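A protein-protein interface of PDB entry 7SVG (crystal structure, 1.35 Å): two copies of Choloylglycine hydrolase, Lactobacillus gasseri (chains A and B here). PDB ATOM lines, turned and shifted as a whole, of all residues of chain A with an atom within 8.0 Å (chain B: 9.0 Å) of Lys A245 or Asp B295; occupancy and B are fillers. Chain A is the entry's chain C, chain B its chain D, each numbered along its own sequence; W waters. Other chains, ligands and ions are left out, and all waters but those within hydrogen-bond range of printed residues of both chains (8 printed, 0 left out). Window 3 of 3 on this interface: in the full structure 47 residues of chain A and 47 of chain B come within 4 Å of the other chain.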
ATOM      1  N   TYR A  15      -8.420  -7.107  18.396  1.00  0.00           N
ATOM      2  CA  TYR A  15      -7.151  -6.527  18.824  1.00  0.00           C
ATOM      3  C   TYR A  15      -6.055  -7.396  18.221  1.00  0.00           C
ATOM      4  O   TYR A  15      -6.033  -8.607  18.445  1.00  0.00           O
ATOM      5  CB  TYR A  15      -7.078  -6.484  20.364  1.00  0.00           C
ATOM      6  CG  TYR A  15      -8.173  -5.582  20.897  1.00  0.00           C
ATOM      7  CD1 TYR A  15      -9.476  -6.056  21.064  1.00  0.00           C
ATOM      8  CD2 TYR A  15      -7.934  -4.229  21.114  1.00  0.00           C
ATOM      9  CE1 TYR A  15     -10.511  -5.201  21.482  1.00  0.00           C
ATOM     10  CE2 TYR A  15      -8.955  -3.371  21.527  1.00  0.00           C
ATOM     11  CZ  TYR A  15     -10.237  -3.867  21.708  1.00  0.00           C
ATOM     12  OH  TYR A  15     -11.241  -3.006  22.125  1.00  0.00           O
ATOM     13  N   VAL A 241     -11.997 -10.009  28.049  1.00  0.00           N
ATOM     14  CA  VAL A 241     -12.167  -8.817  28.871  1.00  0.00           C
ATOM     15  C   VAL A 241     -12.976  -7.786  28.094  1.00  0.00           C
ATOM     16  O   VAL A 241     -13.133  -7.878  26.873  1.00  0.00           O
ATOM     17  CB  VAL A 241     -10.825  -8.236  29.364  1.00  0.00           C
ATOM     18  CG1 VAL A 241     -10.054  -9.277  30.194  1.00  0.00           C
ATOM     19  CG2 VAL A 241      -9.983  -7.746  28.199  1.00  0.00           C
ATOM     20  N   LYS A 242     -13.491  -6.791  28.814  1.00  0.00           N
ATOM     21  CA  LYS A 242     -14.477  -5.862  28.262  1.00  0.00           C
ATOM     22  C   LYS A 242     -13.903  -4.458  28.111  1.00  0.00           C
ATOM     23  O   LYS A 242     -13.300  -3.921  29.046  1.00  0.00           O
ATOM     24  CB  LYS A 242     -15.721  -5.815  29.152  1.00  0.00           C
ATOM     25  N   GLY A 243     -14.132  -3.848  26.950  1.00  0.00           N
ATOM     26  CA  GLY A 243     -13.802  -2.450  26.763  1.00  0.00           C
ATOM     27  C   GLY A 243     -12.420  -2.224  26.170  1.00  0.00           C
ATOM     28  O   GLY A 243     -11.520  -3.066  26.248  1.00  0.00           O
ATOM     29  N   GLU A 244     -12.253  -1.030  25.595  1.00  0.00           N
ATOM     30  CA  GLU A 244     -11.041  -0.706  24.850  1.00  0.00           C
ATOM     31  C   GLU A 244      -9.802  -0.726  25.744  1.00  0.00           C
ATOM     32  O   GLU A 244      -8.793  -1.343  25.395  1.00  0.00           O
ATOM     33  CB  GLU A 244     -11.197   0.646  24.145  1.00  0.00           C
ATOM     34  CG  GLU A 244      -9.951   1.139  23.419  1.00  0.00           C
ATOM     35  CD  GLU A 244      -9.843   0.586  22.009  1.00  0.00           C
ATOM     36  OE1 GLU A 244     -10.626  -0.310  21.672  1.00  0.00           O
ATOM     37  OE2 GLU A 244      -8.985   1.060  21.242  1.00  0.00           O
ATOM     38  N   LYS A 245      -9.849  -0.046  26.897  1.00  0.00           N
ATOM     39  CA  LYS A 245      -8.661   0.019  27.749  1.00  0.00           C
ATOM     40  C   LYS A 245      -8.234  -1.369  28.211  1.00  0.00           C
ATOM     41  O   LYS A 245      -7.042  -1.702  28.188  1.00  0.00           O
ATOM     42  CB  LYS A 245      -8.898   0.936  28.954  1.00  0.00           C
ATOM     43  CG  LYS A 245      -8.952   2.422  28.598  1.00  0.00           C
ATOM     44  CD  LYS A 245      -9.032   3.277  29.870  1.00  0.00           C
ATOM     45  CE  LYS A 245      -9.404   4.717  29.542  1.00  0.00           C
ATOM     46  NZ  LYS A 245      -8.357   5.334  28.697  1.00  0.00           N
ATOM     47  N   ALA A 246      -9.193  -2.194  28.641  1.00  0.00           N
ATOM     48  CA  ALA A 246      -8.836  -3.502  29.182  1.00  0.00           C
ATOM     49  C   ALA A 246      -8.282  -4.417  28.099  1.00  0.00           C
ATOM     50  O   ALA A 246      -7.389  -5.230  28.361  1.00  0.00           O
ATOM     51  CB  ALA A 246     -10.048  -4.150  29.855  1.00  0.00           C
ATOM     52  N   ASN A 247      -8.799  -4.303  26.880  1.00  0.00           N
ATOM     53  CA  ASN A 247      -8.345  -5.188  25.814  1.00  0.00           C
ATOM     54  C   ASN A 247      -6.972  -4.781  25.292  1.00  0.00           C
ATOM     55  O   ASN A 247      -6.123  -5.642  25.020  1.00  0.00           O
ATOM     56  CB  ASN A 247      -9.394  -5.236  24.697  1.00  0.00           C
ATOM     57  CG  ASN A 247     -10.473  -6.264  24.975  1.00  0.00           C
ATOM     58  OD1 ASN A 247     -10.288  -7.453  24.711  1.00  0.00           O
ATOM     59  ND2 ASN A 247     -11.587  -5.821  25.547  1.00  0.00           N
ATOM     60  N   VAL A 248      -6.732  -3.480  25.142  1.00  0.00           N
ATOM     61  CA  VAL A 248      -5.393  -3.026  24.793  1.00  0.00           C
ATOM     62  C   VAL A 248      -4.399  -3.448  25.867  1.00  0.00           C
ATOM     63  O   VAL A 248      -3.281  -3.877  25.566  1.00  0.00           O
ATOM     64  CB  VAL A 248      -5.391  -1.508  24.550  1.00  0.00           C
ATOM     65  CG1 VAL A 248      -3.980  -0.992  24.367  1.00  0.00           C
ATOM     66  CG2 VAL A 248      -6.256  -1.165  23.316  1.00  0.00           C
ATOM     67  N   ALA A 249      -4.798  -3.342  27.140  1.00  0.00           N
ATOM     68  CA  ALA A 249      -3.904  -3.740  28.226  1.00  0.00           C
ATOM     69  C   ALA A 249      -3.617  -5.236  28.180  1.00  0.00           C
ATOM     70  O   ALA A 249      -2.462  -5.653  28.258  1.00  0.00           O
ATOM     71  CB  ALA A 249      -4.498  -3.326  29.571  1.00  0.00           C
ATOM     72  N   LYS A 250      -4.666  -6.053  28.046  1.00  0.00           N
ATOM     73  CA  LYS A 250      -4.489  -7.492  27.881  1.00  0.00           C
ATOM     74  C   LYS A 250      -3.507  -7.793  26.761  1.00  0.00           C
ATOM     75  O   LYS A 250      -2.617  -8.644  26.908  1.00  0.00           O
ATOM     76  CB  LYS A 250      -5.850  -8.141  27.598  1.00  0.00           C
ATOM     77  CG  LYS A 250      -5.777  -9.551  27.025  1.00  0.00           C
ATOM     78  CD  LYS A 250      -7.179 -10.109  26.797  1.00  0.00           C
ATOM     79  CE  LYS A 250      -7.144 -11.408  26.009  1.00  0.00           C
ATOM     80  NZ  LYS A 250      -8.490 -12.046  25.970  1.00  0.00           N
ATOM     81  N   PHE A 251      -3.666  -7.102  25.623  1.00  0.00           N
ATOM     82  CA  PHE A 251      -2.811  -7.331  24.465  1.00  0.00           C
ATOM     83  C   PHE A 251      -1.345  -7.072  24.797  1.00  0.00           C
ATOM     84  O   PHE A 251      -0.480  -7.923  24.560  1.00  0.00           O
ATOM     85  CB  PHE A 251      -3.282  -6.429  23.310  1.00  0.00           C
ATOM     86  CG  PHE A 251      -2.541  -6.677  22.047  1.00  0.00           C
ATOM     87  CD1 PHE A 251      -1.298  -6.102  21.838  1.00  0.00           C
ATOM     88  CD2 PHE A 251      -3.053  -7.544  21.104  1.00  0.00           C
ATOM     89  CE1 PHE A 251      -0.582  -6.361  20.678  1.00  0.00           C
ATOM     90  CE2 PHE A 251      -2.349  -7.810  19.938  1.00  0.00           C
ATOM     91  CZ  PHE A 251      -1.111  -7.214  19.728  1.00  0.00           C
ATOM     92  N   PHE A 252      -1.046  -5.902  25.383  1.00  0.00           N
ATOM     93  CA  PHE A 252       0.331  -5.585  25.743  1.00  0.00           C
ATOM     94  C   PHE A 252       0.842  -6.478  26.876  1.00  0.00           C
ATOM     95  O   PHE A 252       2.041  -6.780  26.931  1.00  0.00           O
ATOM     96  CB  PHE A 252       0.435  -4.100  26.125  1.00  0.00           C
ATOM     97  CG  PHE A 252       0.608  -3.185  24.941  1.00  0.00           C
ATOM     98  CD1 PHE A 252      -0.487  -2.807  24.169  1.00  0.00           C
ATOM     99  CD2 PHE A 252       1.871  -2.740  24.567  1.00  0.00           C
ATOM    100  CE1 PHE A 252      -0.325  -1.972  23.047  1.00  0.00           C
ATOM    101  CE2 PHE A 252       2.046  -1.917  23.453  1.00  0.00           C
ATOM    102  CZ  PHE A 252       0.946  -1.535  22.688  1.00  0.00           C
ATOM    103  N   ASN A 253      -0.039  -6.896  27.787  1.00  0.00           N
ATOM    104  CA  ASN A 253       0.384  -7.804  28.855  1.00  0.00           C
ATOM    105  C   ASN A 253       0.952  -9.089  28.263  1.00  0.00           C
ATOM    106  O   ASN A 253       2.005  -9.577  28.691  1.00  0.00           O
ATOM    107  CB  ASN A 253      -0.804  -8.151  29.758  1.00  0.00           C
ATOM    108  CG  ASN A 253      -1.267  -6.996  30.616  1.00  0.00           C
ATOM    109  OD1 ASN A 253      -0.515  -6.062  30.909  1.00  0.00           O
ATOM    110  ND2 ASN A 253      -2.520  -7.070  31.043  1.00  0.00           N
ATOM    111  N   SER A 282      -6.564  -1.677  17.302  1.00  0.00           N
ATOM    112  CA  SER A 282      -7.946  -1.895  17.708  1.00  0.00           C
ATOM    113  C   SER A 282      -8.851  -1.552  16.526  1.00  0.00           C
ATOM    114  O   SER A 282      -8.959  -0.384  16.138  1.00  0.00           O
ATOM    115  CB  SER A 282      -8.298  -1.003  18.891  1.00  0.00           C
ATOM    116  OG  SER A 282      -9.677  -1.130  19.161  1.00  0.00           O
ATOM    117  N   THR A 285     -11.809   1.126  17.292  1.00  0.00           N
ATOM    118  CA  THR A 285     -11.476   2.545  17.338  1.00  0.00           C
ATOM    119  C   THR A 285     -10.563   2.977  16.203  1.00  0.00           C
ATOM    120  O   THR A 285     -10.146   4.144  16.173  1.00  0.00           O
ATOM    121  CB  THR A 285     -10.809   2.898  18.676  1.00  0.00           C
ATOM    122  OG1 THR A 285      -9.599   2.135  18.814  1.00  0.00           O
ATOM    123  CG2 THR A 285     -11.739   2.595  19.850  1.00  0.00           C
ATOM    124  N   TYR A 289      -1.909   1.490  18.544  1.00  0.00           N
ATOM    125  CA  TYR A 289      -1.195   1.778  19.783  1.00  0.00           C
ATOM    126  C   TYR A 289       0.199   1.174  19.688  1.00  0.00           C
ATOM    127  O   TYR A 289       0.353   0.041  19.221  1.00  0.00           O
ATOM    128  CB  TYR A 289      -1.887   1.070  20.948  1.00  0.00           C
ATOM    129  CG  TYR A 289      -3.297   1.498  21.267  1.00  0.00           C
ATOM    130  CD1 TYR A 289      -4.385   0.977  20.565  1.00  0.00           C
ATOM    131  CD2 TYR A 289      -3.549   2.392  22.306  1.00  0.00           C
ATOM    132  CE1 TYR A 289      -5.686   1.358  20.873  1.00  0.00           C
ATOM    133  CE2 TYR A 289      -4.845   2.774  22.623  1.00  0.00           C
ATOM    134  CZ  TYR A 289      -5.909   2.260  21.900  1.00  0.00           C
ATOM    135  OH  TYR A 289      -7.192   2.629  22.232  1.00  0.00           O
ATOM    136  N   LEU A 298       2.575   4.687  25.886  1.00  0.00           N
ATOM    137  CA  LEU A 298       1.689   4.179  24.843  1.00  0.00           C
ATOM    138  C   LEU A 298       1.332   5.335  23.918  1.00  0.00           C
ATOM    139  O   LEU A 298       0.629   6.264  24.327  1.00  0.00           O
ATOM    140  CB  LEU A 298       0.423   3.631  25.490  1.00  0.00           C
ATOM    141  CG  LEU A 298      -0.226   2.407  24.863  1.00  0.00           C
ATOM    142  CD1 LEU A 298       0.784   1.272  24.774  1.00  0.00           C
ATOM    143  CD2 LEU A 298      -1.437   1.993  25.668  1.00  0.00           C
ATOM    144  N   PHE B 252      10.292  -1.211  32.851  1.00  0.00           N
ATOM    145  CA  PHE B 252       9.046  -1.890  32.519  1.00  0.00           C
ATOM    146  C   PHE B 252       9.276  -3.067  31.572  1.00  0.00           C
ATOM    147  O   PHE B 252       8.552  -4.065  31.648  1.00  0.00           O
ATOM    148  CB  PHE B 252       8.053  -0.886  31.924  1.00  0.00           C
ATOM    149  CG  PHE B 252       7.310  -0.102  32.965  1.00  0.00           C
ATOM    150  CD1 PHE B 252       7.897   0.993  33.587  1.00  0.00           C
ATOM    151  CD2 PHE B 252       6.037  -0.498  33.370  1.00  0.00           C
ATOM    152  CE1 PHE B 252       7.209   1.697  34.589  1.00  0.00           C
ATOM    153  CE2 PHE B 252       5.342   0.203  34.353  1.00  0.00           C
ATOM    154  CZ  PHE B 252       5.935   1.294  34.968  1.00  0.00           C
ATOM    155  N   LYS B 256       7.685  -6.407  32.958  1.00  0.00           N
ATOM    156  CA  LYS B 256       6.591  -6.993  32.188  1.00  0.00           C
ATOM    157  C   LYS B 256       6.966  -8.349  31.610  1.00  0.00           C
ATOM    158  O   LYS B 256       6.082  -9.182  31.407  1.00  0.00           O
ATOM    159  CB  LYS B 256       6.102  -6.030  31.105  1.00  0.00           C
ATOM    160  CG  LYS B 256       5.472  -4.766  31.694  1.00  0.00           C
ATOM    161  CD  LYS B 256       4.291  -5.085  32.614  1.00  0.00           C
ATOM    162  CE  LYS B 256       3.436  -3.838  32.874  1.00  0.00           C
ATOM    163  NZ  LYS B 256       2.324  -4.149  33.827  1.00  0.00           N
ATOM    164  N   THR B 275      -0.282 -10.130  37.798  1.00  0.00           N
ATOM    165  CA  THR B 275       0.323  -8.822  38.057  1.00  0.00           C
ATOM    166  C   THR B 275      -0.741  -7.743  37.896  1.00  0.00           C
ATOM    167  O   THR B 275      -1.122  -7.382  36.776  1.00  0.00           O
ATOM    168  CB  THR B 275       1.507  -8.585  37.124  1.00  0.00           C
ATOM    169  OG1 THR B 275       2.512  -9.582  37.351  1.00  0.00           O
ATOM    170  CG2 THR B 275       2.119  -7.221  37.383  1.00  0.00           C
ATOM    171  N   VAL B 276      -1.213  -7.214  39.033  1.00  0.00           N
ATOM    172  CA  VAL B 276      -2.257  -6.194  39.011  1.00  0.00           C
ATOM    173  C   VAL B 276      -1.698  -4.825  38.663  1.00  0.00           C
ATOM    174  O   VAL B 276      -2.388  -4.018  38.032  1.00  0.00           O
ATOM    175  CB  VAL B 276      -3.049  -6.182  40.330  1.00  0.00           C
ATOM    176  CG1 VAL B 276      -2.147  -5.786  41.469  1.00  0.00           C
ATOM    177  CG2 VAL B 276      -4.201  -5.204  40.240  1.00  0.00           C
ATOM    178  N   TYR B 277      -0.469  -4.517  39.076  1.00  0.00           N
ATOM    179  CA  TYR B 277       0.171  -3.285  38.643  1.00  0.00           C
ATOM    180  C   TYR B 277       1.674  -3.480  38.597  1.00  0.00           C
ATOM    181  O   TYR B 277       2.223  -4.367  39.261  1.00  0.00           O
ATOM    182  CB  TYR B 277      -0.205  -2.080  39.524  1.00  0.00           C
ATOM    183  CG  TYR B 277       0.440  -2.008  40.915  1.00  0.00           C
ATOM    184  CD1 TYR B 277       1.744  -1.554  41.087  1.00  0.00           C
ATOM    185  CD2 TYR B 277      -0.291  -2.330  42.046  1.00  0.00           C
ATOM    186  CE1 TYR B 277       2.325  -1.473  42.374  1.00  0.00           C
ATOM    187  CE2 TYR B 277       0.273  -2.237  43.332  1.00  0.00           C
ATOM    188  CZ  TYR B 277       1.570  -1.804  43.475  1.00  0.00           C
ATOM    189  OH  TYR B 277       2.129  -1.727  44.752  1.00  0.00           O
ATOM    190  N   THR B 278       2.329  -2.634  37.804  1.00  0.00           N
ATOM    191  CA  THR B 278       3.779  -2.506  37.745  1.00  0.00           C
ATOM    192  C   THR B 278       4.129  -1.049  38.011  1.00  0.00           C
ATOM    193  O   THR B 278       3.519  -0.149  37.429  1.00  0.00           O
ATOM    194  CB  THR B 278       4.320  -2.895  36.362  1.00  0.00           C
ATOM    195  OG1 THR B 278       3.961  -4.252  36.079  1.00  0.00           O
ATOM    196  CG2 THR B 278       5.840  -2.752  36.329  1.00  0.00           C
ATOM    197  N   CYS B 290       3.340   4.152  36.928  1.00  0.00           N
ATOM    198  CA  CYS B 290       2.688   2.860  37.091  1.00  0.00           C
ATOM    199  C   CYS B 290       1.700   2.606  35.965  1.00  0.00           C
ATOM    200  O   CYS B 290       1.174   3.530  35.339  1.00  0.00           O
ATOM    201  CB  CYS B 290       1.993   2.729  38.451  1.00  0.00           C
ATOM    202  SG  CYS B 290       0.770   4.020  38.811  1.00  0.00           S
ATOM    203  N   ASN B 291       1.435   1.322  35.734  1.00  0.00           N
ATOM    204  CA  ASN B 291       0.289   0.912  34.934  1.00  0.00           C
ATOM    205  C   ASN B 291      -0.350  -0.317  35.578  1.00  0.00           C
ATOM    206  O   ASN B 291       0.162  -0.862  36.566  1.00  0.00           O
ATOM    207  CB  ASN B 291       0.627   0.789  33.436  1.00  0.00           C
ATOM    208  CG  ASN B 291       1.421  -0.463  33.085  1.00  0.00           C
ATOM    209  OD1 ASN B 291       1.793  -1.275  33.939  1.00  0.00           O
ATOM    210  ND2 ASN B 291       1.676  -0.624  31.790  1.00  0.00           N
ATOM    211  N   PHE B 292      -1.474  -0.756  35.016  1.00  0.00           N
ATOM    212  CA  PHE B 292      -2.323  -1.762  35.637  1.00  0.00           C
ATOM    213  C   PHE B 292      -2.721  -2.822  34.615  1.00  0.00           C
ATOM    214  O   PHE B 292      -2.690  -2.592  33.405  1.00  0.00           O
ATOM    215  CB  PHE B 292      -3.573  -1.120  36.235  1.00  0.00           C
ATOM    216  CG  PHE B 292      -3.271  -0.144  37.345  1.00  0.00           C
ATOM    217  CD1 PHE B 292      -3.014   1.189  37.061  1.00  0.00           C
ATOM    218  CD2 PHE B 292      -3.234  -0.565  38.659  1.00  0.00           C
ATOM    219  CE1 PHE B 292      -2.727   2.086  38.079  1.00  0.00           C
ATOM    220  CE2 PHE B 292      -2.941   0.336  39.690  1.00  0.00           C
ATOM    221  CZ  PHE B 292      -2.693   1.658  39.386  1.00  0.00           C
ATOM    222  N   GLU B 293      -3.126  -3.985  35.134  1.00  0.00           N
ATOM    223  CA  GLU B 293      -3.479  -5.109  34.263  1.00  0.00           C
ATOM    224  C   GLU B 293      -4.566  -4.729  33.267  1.00  0.00           C
ATOM    225  O   GLU B 293      -4.605  -5.268  32.150  1.00  0.00           O
ATOM    226  CB  GLU B 293      -3.982  -6.286  35.104  1.00  0.00           C
ATOM    227  CG  GLU B 293      -4.362  -7.538  34.273  1.00  0.00           C
ATOM    228  CD  GLU B 293      -5.811  -7.534  33.753  1.00  0.00           C
ATOM    229  OE1 GLU B 293      -6.690  -6.920  34.400  1.00  0.00           O
ATOM    230  OE2 GLU B 293      -6.084  -8.158  32.693  1.00  0.00           O
ATOM    231  N   ASN B 294      -5.471  -3.831  33.654  1.00  0.00           N
ATOM    232  CA  ASN B 294      -6.587  -3.442  32.793  1.00  0.00           C
ATOM    233  C   ASN B 294      -6.459  -2.029  32.234  1.00  0.00           C
ATOM    234  O   ASN B 294      -7.431  -1.504  31.674  1.00  0.00           O
ATOM    235  CB  ASN B 294      -7.919  -3.619  33.524  1.00  0.00           C
ATOM    236  CG  ASN B 294      -8.061  -2.682  34.701  1.00  0.00           C
ATOM    237  OD1 ASN B 294      -7.112  -1.994  35.075  1.00  0.00           O
ATOM    238  ND2 ASN B 294      -9.256  -2.640  35.285  1.00  0.00           N
ATOM    239  N   ASP B 295      -5.287  -1.400  32.356  1.00  0.00           N
ATOM    240  CA  ASP B 295      -5.083  -0.065  31.793  1.00  0.00           C
ATOM    241  C   ASP B 295      -3.574   0.124  31.644  1.00  0.00           C
ATOM    242  O   ASP B 295      -2.879   0.370  32.633  1.00  0.00           O
ATOM    243  CB  ASP B 295      -5.687   1.005  32.694  1.00  0.00           C
ATOM    244  CG  ASP B 295      -5.666   2.387  32.054  1.00  0.00           C
ATOM    245  OD1 ASP B 295      -4.970   2.562  31.032  1.00  0.00           O
ATOM    246  OD2 ASP B 295      -6.332   3.301  32.585  1.00  0.00           O
ATOM    247  N   PHE B 296      -3.090   0.023  30.409  1.00  0.00           N
ATOM    248  CA  PHE B 296      -1.656  -0.033  30.169  1.00  0.00           C
ATOM    249  C   PHE B 296      -0.995   1.336  30.103  1.00  0.00           C
ATOM    250  O   PHE B 296       0.237   1.404  30.098  1.00  0.00           O
ATOM    251  CB  PHE B 296      -1.380  -0.824  28.878  1.00  0.00           C
ATOM    252  CG  PHE B 296      -0.080  -1.581  28.892  1.00  0.00           C
ATOM    253  CD1 PHE B 296       0.026  -2.794  29.571  1.00  0.00           C
ATOM    254  CD2 PHE B 296       1.050  -1.076  28.253  1.00  0.00           C
ATOM    255  CE1 PHE B 296       1.235  -3.501  29.584  1.00  0.00           C
ATOM    256  CE2 PHE B 296       2.248  -1.767  28.269  1.00  0.00           C
ATOM    257  CZ  PHE B 296       2.345  -2.977  28.944  1.00  0.00           C
ATOM    258  N   GLU B 297      -1.775   2.421  30.039  1.00  0.00           N
ATOM    259  CA  GLU B 297      -1.213   3.764  29.976  1.00  0.00           C
ATOM    260  C   GLU B 297      -0.310   4.001  31.181  1.00  0.00           C
ATOM    261  O   GLU B 297      -0.691   3.703  32.313  1.00  0.00           O
ATOM    262  CB  GLU B 297      -2.377   4.748  30.017  1.00  0.00           C
ATOM    263  CG  GLU B 297      -2.025   6.168  30.386  1.00  0.00           C
ATOM    264  CD  GLU B 297      -3.116   7.141  29.981  1.00  0.00           C
ATOM    265  OE1 GLU B 297      -2.981   8.348  30.276  1.00  0.00           O
ATOM    266  OE2 GLU B 297      -4.120   6.689  29.389  1.00  0.00           O
ATOM    267  N   LEU B 298       0.886   4.536  30.938  1.00  0.00           N
ATOM    268  CA  LEU B 298       1.816   4.849  32.023  1.00  0.00           C
ATOM    269  C   LEU B 298       1.335   6.124  32.697  1.00  0.00           C
ATOM    270  O   LEU B 298       1.316   7.197  32.080  1.00  0.00           O
ATOM    271  CB  LEU B 298       3.222   5.071  31.476  1.00  0.00           C
ATOM    272  CG  LEU B 298       4.365   4.101  31.763  1.00  0.00           C
ATOM    273  CD1 LEU B 298       5.692   4.790  31.490  1.00  0.00           C
ATOM    274  CD2 LEU B 298       4.312   3.562  33.173  1.00  0.00           C
ATOM    275  N   LYS B 299       0.926   6.011  33.950  1.00  0.00           N
ATOM    276  CA  LYS B 299       0.509   7.163  34.732  1.00  0.00           C
ATOM    277  C   LYS B 299       1.688   7.635  35.570  1.00  0.00           C
ATOM    278  O   LYS B 299       2.550   6.840  35.946  1.00  0.00           O
ATOM    279  CB  LYS B 299      -0.685   6.785  35.602  1.00  0.00           C
ATOM    280  CG  LYS B 299      -1.858   6.262  34.753  1.00  0.00           C
ATOM    281  CD  LYS B 299      -3.207   6.637  35.308  1.00  0.00           C
ATOM    282  CE  LYS B 299      -4.318   6.268  34.334  1.00  0.00           C
ATOM    283  NZ  LYS B 299      -4.860   4.903  34.627  1.00  0.00           N
ATOM    284  N   TYR B 301       3.108  10.341  38.786  1.00  0.00           N
ATOM    285  CA  TYR B 301       2.822  11.115  39.986  1.00  0.00           C
ATOM    286  C   TYR B 301       4.155  11.576  40.552  1.00  0.00           C
ATOM    287  O   TYR B 301       5.152  10.863  40.447  1.00  0.00           O
ATOM    288  CB  TYR B 301       2.054  10.246  40.989  1.00  0.00           C
ATOM    289  CG  TYR B 301       0.829   9.624  40.362  1.00  0.00           C
ATOM    290  CD1 TYR B 301      -0.371  10.322  40.292  1.00  0.00           C
ATOM    291  CD2 TYR B 301       0.882   8.355  39.790  1.00  0.00           C
ATOM    292  CE1 TYR B 301      -1.494   9.758  39.706  1.00  0.00           C
ATOM    293  CE2 TYR B 301      -0.228   7.790  39.211  1.00  0.00           C
ATOM    294  CZ  TYR B 301      -1.408   8.496  39.161  1.00  0.00           C
ATOM    295  OH  TYR B 301      -2.521   7.939  38.576  1.00  0.00           O
HETATM  296  O   HOH W   1       3.352  -8.317  30.896  1.00  0.00           O
HETATM  297  O   HOH W   2      -5.695   4.240  29.017  1.00  0.00           O
HETATM  298  O   HOH W   3      -7.549  -6.417  30.961  1.00  0.00           O
HETATM  299  O   HOH W   4       1.479  -7.023  32.605  1.00  0.00           O
HETATM  300  O   HOH W   5       1.356   5.804  28.344  1.00  0.00           O
HETATM  301  O   HOH W   6      -6.689   5.541  31.434  1.00  0.00           O
HETATM  302  O   HOH W   7      -0.337  -4.099  32.799  1.00  0.00           O
HETATM  303  O   HOH W   8      -4.745  -0.010  28.116  1.00  0.00           O
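Positions printed for both chains: 252 and 298. Of the 10 pairs that touch across the chains among the printed residues, none has its exchanged pair printed and touching as well.
The side-chain amide nitrogen (ND2) of Asn A253 lies close to the backbone carbonyl oxygen (O) of Ala A249, at 3.1 Å. The backbone NH of Glu B293 lies within hydrogen-bond range of the backbone carbonyl oxygen of Val B276, 3.0 Å away. O of Phe B296 sits at hydrogen-bond distance from ND2 of Asn B291, 3.0 Å away. OD1 of Asp B295 lies close to N of Glu B297, 3.3 Å away. OD2 of Asp B295 is in salt-bridge range of NZ of Lys B299 (3.0 Å).
Lys A245 touches Asn B294 (O to O, 3.5 Å). Lys A245 touches Asp B295. Asn B294 touches Ala A246. CB of Ala A249 touches O of Glu B293, at 3.2 Å. Asn B294 touches Ala A249. CB of Ala A249 touches N of Asp B295, 3.5 Å away. Phe B296 touches Ala A249. Phe B296 touches Phe A252. Asn A253 touches Phe B296 (OD1 to CE1, 3.4 Å).
Water W6 lies within hydrogen-bond range of the side-chain carboxylate of Asp B295, the side-chain amino group of Lys A245 and the side-chain carboxylate of Glu B297. Water W2 lies within hydrogen-bond range of OD1 of Asp B295 (2.7 Å), NZ of Lys A245 (2.9 Å) and OE2 of Glu B297 (2.9 Å). Water W7 lies within hydrogen-bond range of the side-chain amide oxygen of Asn A253 (2.7 Å), the side-chain amino group of Lys B256 (2.9 Å) and the backbone carbonyl oxygen of Phe B292 (2.9 Å). Water W4 lies within hydrogen-bond range of the side-chain amide oxygen (OD1) of Asn A253 (2.8 Å) and the side-chain amino group (NZ) of Lys B256 (3.2 Å). Water W3 bridges OE2 of Glu B293 and O of Ala A246. Water W1 lies within hydrogen-bond range of O of Asn A253 (2.9 Å) and O of Lys B256 (2.9 Å).
Lys A245 touches just these residues of chain B: Asn B294 (3.5 Å) and Asp B295 (3.8 Å). Of chain B, only Asn B294 (3.5 Å) comes within 4 Å of Ala A246. Of the printed residues of chain B, Phe A252 touches Phe B296 (3.6 Å). Of the printed residues of chain B, Asn A253 touches Glu B293 and Phe B296. Of the printed residues of chain A, Asn B294 touches Lys A245 (3.5 Å), Ala A246 (3.5 Å) and Ala A249 (3.6 Å). Asp B295 touches two residues of chain A. Printed residues of chain A within 4 Å of Phe B296: Ala A249 (3.7 Å), Phe A252 (3.6 Å) and Asn A253 (3.4 Å). The nearest residue of chain B that does not touch Lys A245 is Glu B297 (4.5 Å). The nearest residue of chain A that does not touch Asp B295 is Ala A246 (5.2 Å). The nearest printed residue of chain A that does not touch Glu B293 is Lys A250 (4.2 Å).
The side-chain amide nitrogen (ND2) of Asn A253 sits at hydrogen-bond distance from the backbone carbonyl oxygen (O) of Glu B293 (3.0 Å).
Printed residues of chain B that touch a printed residue of chain A: Glu B293, Asn B294, Asp B295 and Phe B296. Hydrophobic or aromatic side chains of chain B within 4 Å of the printed part of chain A: Phe B296.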
